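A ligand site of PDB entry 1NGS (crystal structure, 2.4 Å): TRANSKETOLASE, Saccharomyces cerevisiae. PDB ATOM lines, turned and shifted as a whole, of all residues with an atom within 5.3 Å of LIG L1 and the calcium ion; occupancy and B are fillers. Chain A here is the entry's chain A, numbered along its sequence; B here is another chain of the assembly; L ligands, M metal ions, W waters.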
ATOM      1  N   ALA A  33     -37.724  30.052  11.149  1.00  0.00           N
ATOM      2  CA  ALA A  33     -38.127  28.793  10.522  1.00  0.00           C
ATOM      3  C   ALA A  33     -39.364  28.181  11.179  1.00  0.00           C
ATOM      4  O   ALA A  33     -40.243  27.686  10.479  1.00  0.00           O
ATOM      5  CB  ALA A  33     -36.975  27.807  10.492  1.00  0.00           C
ATOM      6  N   ASN A  67     -32.663  20.868  10.005  1.00  0.00           N
ATOM      7  CA  ASN A  67     -32.385  22.260  10.383  1.00  0.00           C
ATOM      8  C   ASN A  67     -32.696  22.418  11.878  1.00  0.00           C
ATOM      9  O   ASN A  67     -33.630  23.117  12.277  1.00  0.00           O
ATOM     10  CB  ASN A  67     -33.208  23.231   9.537  1.00  0.00           C
ATOM     11  CG  ASN A  67     -34.687  22.854   9.403  1.00  0.00           C
ATOM     12  OD1 ASN A  67     -35.481  23.670   8.947  1.00  0.00           O
ATOM     13  ND2 ASN A  67     -35.050  21.621   9.755  1.00  0.00           N
ATOM     14  N   HIS A  69     -31.782  24.203  14.380  1.00  0.00           N
ATOM     15  CA  HIS A  69     -31.992  25.491  15.021  1.00  0.00           C
ATOM     16  C   HIS A  69     -33.471  25.789  15.213  1.00  0.00           C
ATOM     17  O   HIS A  69     -33.852  26.556  16.117  1.00  0.00           O
ATOM     18  CB  HIS A  69     -31.241  26.628  14.298  1.00  0.00           C
ATOM     19  CG  HIS A  69     -31.636  26.834  12.852  1.00  0.00           C
ATOM     20  ND1 HIS A  69     -30.935  26.269  11.813  1.00  0.00           N
ATOM     21  CD2 HIS A  69     -32.621  27.570  12.302  1.00  0.00           C
ATOM     22  CE1 HIS A  69     -31.481  26.654  10.665  1.00  0.00           C
ATOM     23  NE2 HIS A  69     -32.506  27.444  10.936  1.00  0.00           N
ATOM     24  N   GLY A 116     -27.924  20.176  14.917  1.00  0.00           N
ATOM     25  CA  GLY A 116     -27.473  21.500  15.281  1.00  0.00           C
ATOM     26  C   GLY A 116     -26.538  21.740  14.124  1.00  0.00           C
ATOM     27  O   GLY A 116     -26.702  22.722  13.403  1.00  0.00           O
ATOM     28  N   PRO A 117     -25.516  20.871  13.941  1.00  0.00           N
ATOM     29  CA  PRO A 117     -24.551  20.978  12.842  1.00  0.00           C
ATOM     30  C   PRO A 117     -25.349  20.736  11.555  1.00  0.00           C
ATOM     31  O   PRO A 117     -26.034  19.698  11.419  1.00  0.00           O
ATOM     32  CB  PRO A 117     -23.613  19.795  13.103  1.00  0.00           C
ATOM     33  CG  PRO A 117     -23.620  19.666  14.565  1.00  0.00           C
ATOM     34  CD  PRO A 117     -25.076  19.848  14.917  1.00  0.00           C
ATOM     35  N   LEU A 118     -25.287  21.687  10.637  1.00  0.00           N
ATOM     36  CA  LEU A 118     -26.037  21.554   9.397  1.00  0.00           C
ATOM     37  C   LEU A 118     -25.510  20.420   8.538  1.00  0.00           C
ATOM     38  O   LEU A 118     -24.333  20.071   8.578  1.00  0.00           O
ATOM     39  CB  LEU A 118     -26.012  22.858   8.604  1.00  0.00           C
ATOM     40  CG  LEU A 118     -26.710  24.031   9.287  1.00  0.00           C
ATOM     41  CD1 LEU A 118     -26.696  25.293   8.423  1.00  0.00           C
ATOM     42  CD2 LEU A 118     -28.117  23.599   9.561  1.00  0.00           C
ATOM     43  N   GLY A 156     -33.205  23.064   5.405  1.00  0.00           N
ATOM     44  CA  GLY A 156     -33.109  24.420   4.922  1.00  0.00           C
ATOM     45  C   GLY A 156     -31.995  24.628   3.922  1.00  0.00           C
ATOM     46  O   GLY A 156     -31.319  23.678   3.507  1.00  0.00           O
ATOM     47  N   ASP A 157     -31.765  25.880   3.566  1.00  0.00           N
ATOM     48  CA  ASP A 157     -30.717  26.184   2.604  1.00  0.00           C
ATOM     49  C   ASP A 157     -29.342  25.784   3.145  1.00  0.00           C
ATOM     50  O   ASP A 157     -28.501  25.282   2.391  1.00  0.00           O
ATOM     51  CB  ASP A 157     -30.811  27.650   2.186  1.00  0.00           C
ATOM     52  CG  ASP A 157     -32.213  28.053   1.771  1.00  0.00           C
ATOM     53  OD1 ASP A 157     -33.011  28.454   2.632  1.00  0.00           O
ATOM     54  OD2 ASP A 157     -32.507  27.950   0.568  1.00  0.00           O
ATOM     55  N   GLY A 158     -29.143  25.914   4.458  1.00  0.00           N
ATOM     56  CA  GLY A 158     -27.872  25.552   5.066  1.00  0.00           C
ATOM     57  C   GLY A 158     -27.520  24.093   4.880  1.00  0.00           C
ATOM     58  O   GLY A 158     -26.375  23.765   4.574  1.00  0.00           O
ATOM     59  N   CYS A 159     -28.506  23.216   5.090  1.00  0.00           N
ATOM     60  CA  CYS A 159     -28.297  21.775   4.923  1.00  0.00           C
ATOM     61  C   CYS A 159     -27.936  21.436   3.472  1.00  0.00           C
ATOM     62  O   CYS A 159     -27.098  20.583   3.228  1.00  0.00           O
ATOM     63  CB  CYS A 159     -29.535  20.980   5.367  1.00  0.00           C
ATOM     64  SG  CYS A 159     -29.797  20.941   7.154  1.00  0.00           S
ATOM     65  N   GLU A 162     -24.042  22.306   2.585  1.00  0.00           N
ATOM     66  CA  GLU A 162     -23.007  21.445   3.153  1.00  0.00           C
ATOM     67  C   GLU A 162     -22.763  20.195   2.303  1.00  0.00           C
ATOM     68  O   GLU A 162     -23.688  19.411   2.042  1.00  0.00           O
ATOM     69  CB  GLU A 162     -23.372  21.050   4.592  1.00  0.00           C
ATOM     70  CG  GLU A 162     -23.319  22.210   5.594  1.00  0.00           C
ATOM     71  CD  GLU A 162     -21.911  22.484   6.089  1.00  0.00           C
ATOM     72  OE1 GLU A 162     -20.944  22.107   5.410  1.00  0.00           O
ATOM     73  OE2 GLU A 162     -21.777  23.039   7.191  1.00  0.00           O
ATOM     74  N   ASP A 185     -37.437  23.818   3.188  1.00  0.00           N
ATOM     75  CA  ASP A 185     -37.857  25.158   3.567  1.00  0.00           C
ATOM     76  C   ASP A 185     -37.155  26.159   2.655  1.00  0.00           C
ATOM     77  O   ASP A 185     -36.062  26.648   2.953  1.00  0.00           O
ATOM     78  CB  ASP A 185     -37.477  25.423   5.041  1.00  0.00           C
ATOM     79  CG  ASP A 185     -38.143  26.661   5.618  1.00  0.00           C
ATOM     80  OD1 ASP A 185     -39.098  27.188   5.014  1.00  0.00           O
ATOM     81  OD2 ASP A 185     -37.702  27.113   6.699  1.00  0.00           O
ATOM     82  N   ASN A 187     -37.000  29.385   1.830  1.00  0.00           N
ATOM     83  CA  ASN A 187     -37.368  30.725   2.249  1.00  0.00           C
ATOM     84  C   ASN A 187     -36.512  31.896   1.783  1.00  0.00           C
ATOM     85  O   ASN A 187     -36.829  33.050   2.101  1.00  0.00           O
ATOM     86  CB  ASN A 187     -37.575  30.791   3.762  1.00  0.00           C
ATOM     87  CG  ASN A 187     -36.327  30.461   4.551  1.00  0.00           C
ATOM     88  OD1 ASN A 187     -35.233  30.359   3.983  1.00  0.00           O
ATOM     89  ND2 ASN A 187     -36.478  30.301   5.863  1.00  0.00           N
ATOM     90  N   LYS A 188     -35.446  31.608   1.053  1.00  0.00           N
ATOM     91  CA  LYS A 188     -34.565  32.638   0.487  1.00  0.00           C
ATOM     92  C   LYS A 188     -33.695  33.426   1.470  1.00  0.00           C
ATOM     93  O   LYS A 188     -33.121  34.459   1.098  1.00  0.00           O
ATOM     94  CB  LYS A 188     -35.379  33.621  -0.360  1.00  0.00           C
ATOM     95  CG  LYS A 188     -35.797  33.126  -1.755  1.00  0.00           C
ATOM     96  CD  LYS A 188     -37.000  32.151  -1.796  1.00  0.00           C
ATOM     97  CE  LYS A 188     -37.495  31.981  -3.248  1.00  0.00           C
ATOM     98  NZ  LYS A 188     -37.961  30.611  -3.653  1.00  0.00           N
ATOM     99  N   ILE A 189     -33.553  32.931   2.690  1.00  0.00           N
ATOM    100  CA  ILE A 189     -32.782  33.637   3.711  1.00  0.00           C
ATOM    101  C   ILE A 189     -31.892  32.689   4.483  1.00  0.00           C
ATOM    102  O   ILE A 189     -32.207  31.518   4.642  1.00  0.00           O
ATOM    103  CB  ILE A 189     -33.752  34.351   4.720  1.00  0.00           C
ATOM    104  CG1 ILE A 189     -34.225  35.705   4.154  1.00  0.00           C
ATOM    105  CG2 ILE A 189     -33.132  34.496   6.122  1.00  0.00           C
ATOM    106  CD1 ILE A 189     -33.235  36.829   4.317  1.00  0.00           C
ATOM    107  N   THR A 190     -30.711  33.189   4.841  1.00  0.00           N
ATOM    108  CA  THR A 190     -29.763  32.466   5.672  1.00  0.00           C
ATOM    109  C   THR A 190     -29.188  33.576   6.555  1.00  0.00           C
ATOM    110  O   THR A 190     -29.615  34.732   6.440  1.00  0.00           O
ATOM    111  CB  THR A 190     -28.658  31.739   4.854  1.00  0.00           C
ATOM    112  OG1 THR A 190     -27.854  32.681   4.136  1.00  0.00           O
ATOM    113  CG2 THR A 190     -29.289  30.759   3.876  1.00  0.00           C
ATOM    114  N   ILE A 191     -28.240  33.262   7.425  1.00  0.00           N
ATOM    115  CA  ILE A 191     -27.668  34.269   8.311  1.00  0.00           C
ATOM    116  C   ILE A 191     -27.116  35.548   7.636  1.00  0.00           C
ATOM    117  O   ILE A 191     -27.534  36.655   7.987  1.00  0.00           O
ATOM    118  CB  ILE A 191     -26.608  33.621   9.230  1.00  0.00           C
ATOM    119  CG1 ILE A 191     -27.284  32.641  10.189  1.00  0.00           C
ATOM    120  CG2 ILE A 191     -25.817  34.677   9.983  1.00  0.00           C
ATOM    121  CD1 ILE A 191     -26.326  31.952  11.087  1.00  0.00           C
ATOM    122  N   ILE A 250     -39.725  33.320   5.864  1.00  0.00           N
ATOM    123  CA  ILE A 250     -39.091  33.228   7.180  1.00  0.00           C
ATOM    124  C   ILE A 250     -39.790  34.220   8.108  1.00  0.00           C
ATOM    125  O   ILE A 250     -40.039  35.354   7.714  1.00  0.00           O
ATOM    126  CB  ILE A 250     -37.541  33.518   7.106  1.00  0.00           C
ATOM    127  CG1 ILE A 250     -36.845  33.044   8.375  1.00  0.00           C
ATOM    128  CG2 ILE A 250     -37.240  35.013   6.908  1.00  0.00           C
ATOM    129  CD1 ILE A 250     -35.361  33.126   8.273  1.00  0.00           C
ATOM    130  N   HIS A 263     -34.134  35.432  11.775  1.00  0.00           N
ATOM    131  CA  HIS A 263     -33.516  34.110  11.763  1.00  0.00           C
ATOM    132  C   HIS A 263     -33.143  33.600  13.148  1.00  0.00           C
ATOM    133  O   HIS A 263     -33.583  32.514  13.546  1.00  0.00           O
ATOM    134  CB  HIS A 263     -32.282  34.008  10.833  1.00  0.00           C
ATOM    135  CG  HIS A 263     -31.300  32.937  11.245  1.00  0.00           C
ATOM    136  ND1 HIS A 263     -31.505  31.593  11.030  1.00  0.00           N
ATOM    137  CD2 HIS A 263     -30.145  33.027  11.944  1.00  0.00           C
ATOM    138  CE1 HIS A 263     -30.537  30.904  11.577  1.00  0.00           C
ATOM    139  NE2 HIS A 263     -29.682  31.747  12.146  1.00  0.00           N
ATOM    140  N   ALA B 381     -18.243  31.915   6.350  1.00  0.00           N
ATOM    141  CA  ALA B 381     -19.112  30.835   5.892  1.00  0.00           C
ATOM    142  C   ALA B 381     -20.497  31.083   6.505  1.00  0.00           C
ATOM    143  O   ALA B 381     -20.901  30.385   7.440  1.00  0.00           O
ATOM    144  CB  ALA B 381     -18.576  29.470   6.342  1.00  0.00           C
ATOM    145  N   ASP B 382     -21.180  32.103   5.993  1.00  0.00           N
ATOM    146  CA  ASP B 382     -22.504  32.503   6.436  1.00  0.00           C
ATOM    147  C   ASP B 382     -22.618  32.910   7.912  1.00  0.00           C
ATOM    148  O   ASP B 382     -23.650  32.680   8.530  1.00  0.00           O
ATOM    149  CB  ASP B 382     -23.552  31.426   6.119  1.00  0.00           C
ATOM    150  CG  ASP B 382     -24.964  31.984   5.996  1.00  0.00           C
ATOM    151  OD1 ASP B 382     -25.185  32.954   5.260  1.00  0.00           O
ATOM    152  OD2 ASP B 382     -25.878  31.469   6.657  1.00  0.00           O
ATOM    153  N   LEU B 383     -21.594  33.557   8.455  1.00  0.00           N
ATOM    154  CA  LEU B 383     -21.634  33.975   9.860  1.00  0.00           C
ATOM    155  C   LEU B 383     -21.012  35.347  10.075  1.00  0.00           C
ATOM    156  O   LEU B 383     -20.568  35.692  11.167  1.00  0.00           O
ATOM    157  CB  LEU B 383     -20.920  32.964  10.749  1.00  0.00           C
ATOM    158  CG  LEU B 383     -21.665  31.691  11.165  1.00  0.00           C
ATOM    159  CD1 LEU B 383     -20.667  30.720  11.774  1.00  0.00           C
ATOM    160  CD2 LEU B 383     -22.790  32.014  12.136  1.00  0.00           C
ATOM    161  N   ILE B 416     -22.697  28.290   3.701  1.00  0.00           N
ATOM    162  CA  ILE B 416     -22.433  27.276   4.717  1.00  0.00           C
ATOM    163  C   ILE B 416     -21.596  26.193   4.021  1.00  0.00           C
ATOM    164  O   ILE B 416     -22.108  25.155   3.608  1.00  0.00           O
ATOM    165  CB  ILE B 416     -23.772  26.706   5.299  1.00  0.00           C
ATOM    166  CG1 ILE B 416     -24.578  27.801   5.991  1.00  0.00           C
ATOM    167  CG2 ILE B 416     -23.485  25.679   6.361  1.00  0.00           C
ATOM    168  CD1 ILE B 416     -25.476  28.585   5.078  1.00  0.00           C
ATOM    169  N   GLU B 418     -17.873  25.203   5.048  1.00  0.00           N
ATOM    170  CA  GLU B 418     -16.598  25.295   5.758  1.00  0.00           C
ATOM    171  C   GLU B 418     -15.400  24.602   5.107  1.00  0.00           C
ATOM    172  O   GLU B 418     -14.328  25.202   4.970  1.00  0.00           O
ATOM    173  CB  GLU B 418     -16.784  24.849   7.215  1.00  0.00           C
ATOM    174  CG  GLU B 418     -17.704  25.792   8.036  1.00  0.00           C
ATOM    175  CD  GLU B 418     -19.174  25.367   8.039  1.00  0.00           C
ATOM    176  OE1 GLU B 418     -19.493  24.270   7.571  1.00  0.00           O
ATOM    177  OE2 GLU B 418     -20.012  26.135   8.536  1.00  0.00           O
ATOM    178  N   PHE B 442     -17.500  29.258  13.307  1.00  0.00           N
ATOM    179  CA  PHE B 442     -17.445  28.993  14.742  1.00  0.00           C
ATOM    180  C   PHE B 442     -16.360  27.933  14.928  1.00  0.00           C
ATOM    181  O   PHE B 442     -16.301  26.982  14.145  1.00  0.00           O
ATOM    182  CB  PHE B 442     -18.788  28.427  15.230  1.00  0.00           C
ATOM    183  CG  PHE B 442     -19.932  29.425  15.259  1.00  0.00           C
ATOM    184  CD1 PHE B 442     -19.701  30.796  15.396  1.00  0.00           C
ATOM    185  CD2 PHE B 442     -21.254  28.982  15.196  1.00  0.00           C
ATOM    186  CE1 PHE B 442     -20.769  31.699  15.493  1.00  0.00           C
ATOM    187  CE2 PHE B 442     -22.321  29.885  15.293  1.00  0.00           C
ATOM    188  CZ  PHE B 442     -22.079  31.240  15.440  1.00  0.00           C
ATOM    189  N   PHE B 445     -16.917  24.308  14.169  1.00  0.00           N
ATOM    190  CA  PHE B 445     -17.160  23.891  12.808  1.00  0.00           C
ATOM    191  C   PHE B 445     -15.955  23.942  11.887  1.00  0.00           C
ATOM    192  O   PHE B 445     -16.040  23.583  10.708  1.00  0.00           O
ATOM    193  CB  PHE B 445     -18.403  24.592  12.304  1.00  0.00           C
ATOM    194  CG  PHE B 445     -19.623  24.290  13.144  1.00  0.00           C
ATOM    195  CD1 PHE B 445     -19.910  22.985  13.520  1.00  0.00           C
ATOM    196  CD2 PHE B 445     -20.476  25.308  13.549  1.00  0.00           C
ATOM    197  CE1 PHE B 445     -21.009  22.686  14.300  1.00  0.00           C
ATOM    198  CE2 PHE B 445     -21.589  25.020  14.333  1.00  0.00           C
ATOM    199  CZ  PHE B 445     -21.862  23.705  14.705  1.00  0.00           C
ATOM    200  N   TYR B 448     -15.247  20.610  10.458  1.00  0.00           N
ATOM    201  CA  TYR B 448     -15.876  20.178   9.221  1.00  0.00           C
ATOM    202  C   TYR B 448     -14.863  20.300   8.089  1.00  0.00           C
ATOM    203  O   TYR B 448     -14.962  19.603   7.065  1.00  0.00           O
ATOM    204  CB  TYR B 448     -17.053  21.091   8.890  1.00  0.00           C
ATOM    205  CG  TYR B 448     -18.410  20.552   9.261  1.00  0.00           C
ATOM    206  CD1 TYR B 448     -18.710  20.178  10.585  1.00  0.00           C
ATOM    207  CD2 TYR B 448     -19.410  20.441   8.304  1.00  0.00           C
ATOM    208  CE1 TYR B 448     -19.969  19.713  10.913  1.00  0.00           C
ATOM    209  CE2 TYR B 448     -20.660  19.987   8.631  1.00  0.00           C
ATOM    210  CZ  TYR B 448     -20.935  19.618   9.922  1.00  0.00           C
ATOM    211  OH  TYR B 448     -22.201  19.153  10.184  1.00  0.00           O
ATOM    212  N   HIS B 481     -22.620  22.933  19.701  1.00  0.00           N
ATOM    213  CA  HIS B 481     -21.840  24.100  19.269  1.00  0.00           C
ATOM    214  C   HIS B 481     -20.627  24.473  20.071  1.00  0.00           C
ATOM    215  O   HIS B 481     -19.801  25.261  19.607  1.00  0.00           O
ATOM    216  CB  HIS B 481     -22.698  25.345  19.188  1.00  0.00           C
ATOM    217  CG  HIS B 481     -23.711  25.310  18.083  1.00  0.00           C
ATOM    218  ND1 HIS B 481     -24.513  24.219  17.862  1.00  0.00           N
ATOM    219  CD2 HIS B 481     -24.044  26.225  17.157  1.00  0.00           C
ATOM    220  CE1 HIS B 481     -25.299  24.464  16.831  1.00  0.00           C
ATOM    221  NE2 HIS B 481     -25.043  25.671  16.385  1.00  0.00           N
HETATM  222  N1  LIG L   1     -22.407  25.373   9.863  1.00  0.00           N
HETATM  223  C1  LIG L   1     -22.721  24.231  10.493  1.00  0.00           C
HETATM  224  C2  LIG L   1     -22.082  22.998  10.042  1.00  0.00           C
HETATM  225  N2  LIG L   1     -23.540  24.222  11.520  1.00  0.00           N
HETATM  226  C3  LIG L   1     -24.159  25.394  11.936  1.00  0.00           C
HETATM  227  N3  LIG L   1     -24.950  25.281  13.010  1.00  0.00           N
HETATM  228  C4  LIG L   1     -23.830  26.640  11.321  1.00  0.00           C
HETATM  229  C5  LIG L   1     -22.953  26.562  10.283  1.00  0.00           C
HETATM  230  C6  LIG L   1     -24.297  27.975  11.867  1.00  0.00           C
HETATM  231  N4  LIG L   1     -25.727  28.254  11.391  1.00  0.00           N
HETATM  232  C7  LIG L   1     -26.864  27.909  12.023  1.00  0.00           C
HETATM  233  S1  LIG L   1     -28.262  28.134  11.078  1.00  0.00           S
HETATM  234  C8  LIG L   1     -27.289  28.778   9.852  1.00  0.00           C
HETATM  235  C9  LIG L   1     -25.970  28.793  10.226  1.00  0.00           C
HETATM  236  C10 LIG L   1     -24.861  29.357   9.453  1.00  0.00           C
HETATM  237  C11 LIG L   1     -27.888  29.287   8.575  1.00  0.00           C
HETATM  238  C12 LIG L   1     -29.351  29.139   8.495  1.00  0.00           C
HETATM  239  O1  LIG L   1     -29.584  28.597   7.201  1.00  0.00           O
HETATM  240  P1  LIG L   1     -30.872  27.768   7.012  1.00  0.00           P
HETATM  241  O2  LIG L   1     -30.740  26.263   6.976  1.00  0.00           O
HETATM  242  O3  LIG L   1     -31.312  28.438   5.802  1.00  0.00           O
HETATM  243  O4  LIG L   1     -32.012  28.375   7.980  1.00  0.00           O
HETATM  244  P2  LIG L   1     -32.991  29.622   8.233  1.00  0.00           P
HETATM  245  O5  LIG L   1     -33.850  29.339   7.076  1.00  0.00           O
HETATM  246  O6  LIG L   1     -33.659  29.321   9.512  1.00  0.00           O
HETATM  247  O7  LIG L   1     -32.199  30.883   8.299  1.00  0.00           O
HETATM  248  C1  LG2 L   2     -27.968  30.929  14.664  1.00  0.00           C
HETATM  249  O1  LG2 L   2     -28.182  29.954  13.930  1.00  0.00           O
HETATM  250  C2  LG2 L   2     -26.837  30.923  15.686  1.00  0.00           C
HETATM  251  O2  LG2 L   2     -26.716  29.632  16.333  1.00  0.00           O
HETATM  252  C3  LG2 L   2     -27.149  31.984  16.734  1.00  0.00           C
HETATM  253  O3  LG2 L   2     -28.208  32.852  16.263  1.00  0.00           O
HETATM  254  C4  LG2 L   2     -25.910  32.824  16.928  1.00  0.00           C
HETATM  255  O4  LG2 L   2     -26.203  33.732  17.989  1.00  0.00           O
HETATM  256  P1  LG2 L   2     -25.060  34.629  18.254  1.00  0.00           P
HETATM  257  O5  LG2 L   2     -25.562  35.930  19.025  1.00  0.00           O
HETATM  258  O6  LG2 L   2     -24.405  35.045  16.863  1.00  0.00           O
HETATM  259  O7  LG2 L   2     -23.988  33.848  19.147  1.00  0.00           O
HETATM  260 CA    CA M   1     -33.205  29.414   4.550  1.00  0.00          CA
HETATM  261  O   HOH W   1     -30.692  23.475   7.238  1.00  0.00           O
HETATM  262  O   HOH W   2     -27.631  26.519  14.976  1.00  0.00           O
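The side-chain carboxylate (OD1) of Asp 157 is bound to the calcium ion, 2.2 Å away. The calcium ion is bound by OD1 of Asn 187 (2.3 Å). The backbone carbonyl oxygen (O) of Ile 189 is bound to the calcium ion (2.3 Å). The calcium ion is bound by O3 of LIG L1, at 2.5 Å. The calcium ion is bound by an oxygen (O5) of LIG L1 (2.6 Å).
NE2 of His 69 is in hydrogen-bond range of O6 of LIG L1 (2.6 Å). O7 of LIG L1 sits at hydrogen-bond distance from ND1 of His 263 (2.9 Å). A nitrogen (N1) of LIG L1 is in hydrogen-bond range of the side-chain carboxylate (OE2) of Glu 418 of chain B. O of Gly 116 sits at hydrogen-bond distance from N3 of LIG L1, 3.1 Å away. The backbone NH of Leu 118 sits at hydrogen-bond distance from a nitrogen (N2) of LIG L1. An oxygen (O3) of LIG L1 sits close to the backbone NH (N) of Asp 157, 3.4 Å away. NE2 of His 263 is in hydrogen-bond range of O1 of LG2 L2 (2.9 Å). The backbone NH (N) of Gly 158 is in hydrogen-bond range of an oxygen (O2) of LIG L1, 3.0 Å away. A nitrogen (N3) of LIG L1 lies within hydrogen-bond range of a ring nitrogen (NE2) of His 481 of chain B, at 3.4 Å.
Three residues have an atom within 4 Å of the calcium ion: Asp 157, Asn 187 and Ile 189.
The side-chain hydroxyl (OH) of Tyr 448 of chain B is in hydrogen-bond range of the backbone carbonyl oxygen (O) of Leu 118 (2.8 Å). OE1 of Glu 418 of chain B sits close to OE2 of Glu 162, 2.6 Å away. The backbone NH of Ile 191 sits at hydrogen-bond distance from the side-chain carboxylate of Asp 382 of chain B, at 3.1 Å. OD1 of Asp 382 of chain B sits at hydrogen-bond distance from OG1 of Thr 190 (2.9 Å).
Water W1 lies within hydrogen-bond range of the side-chain sulfur of Cys 159, an oxygen (O2) of LIG L1 and the backbone NH of Gly 156.
Merely in contact with LIG L1: Ala 33 (3.8 Å), Pro 117 (3.6 Å), Gly 156 (3.6 Å), Glu 162 (2.9 Å), Thr 190 (3.6 Å), Ile 191 (3.3 Å), Ile 250 (3.9 Å), Asp 382 of chain B (3.5 Å), Ile 416 of chain B (3.7 Å), Phe 445 of chain B (3.5 Å) and Tyr 448 of chain B (3.6 Å). 21 residues have an atom within 4 Å of LIG L1: Ala 33, His 69, Gly 116, Pro 117, Leu 118, Gly 156, Asp 157, Gly 158, Glu 162, Asn 187, Ile 189, Thr 190, Ile 191, Ile 250, His 263, Asp 382 of chain B, Ile 416 of chain B, Glu 418 of chain B, Phe 445 of chain B, Tyr 448 of chain B and His 481 of chain B. The nearest printed residue that does not touch LIG L1 is Cys 159 (4.2 Å).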
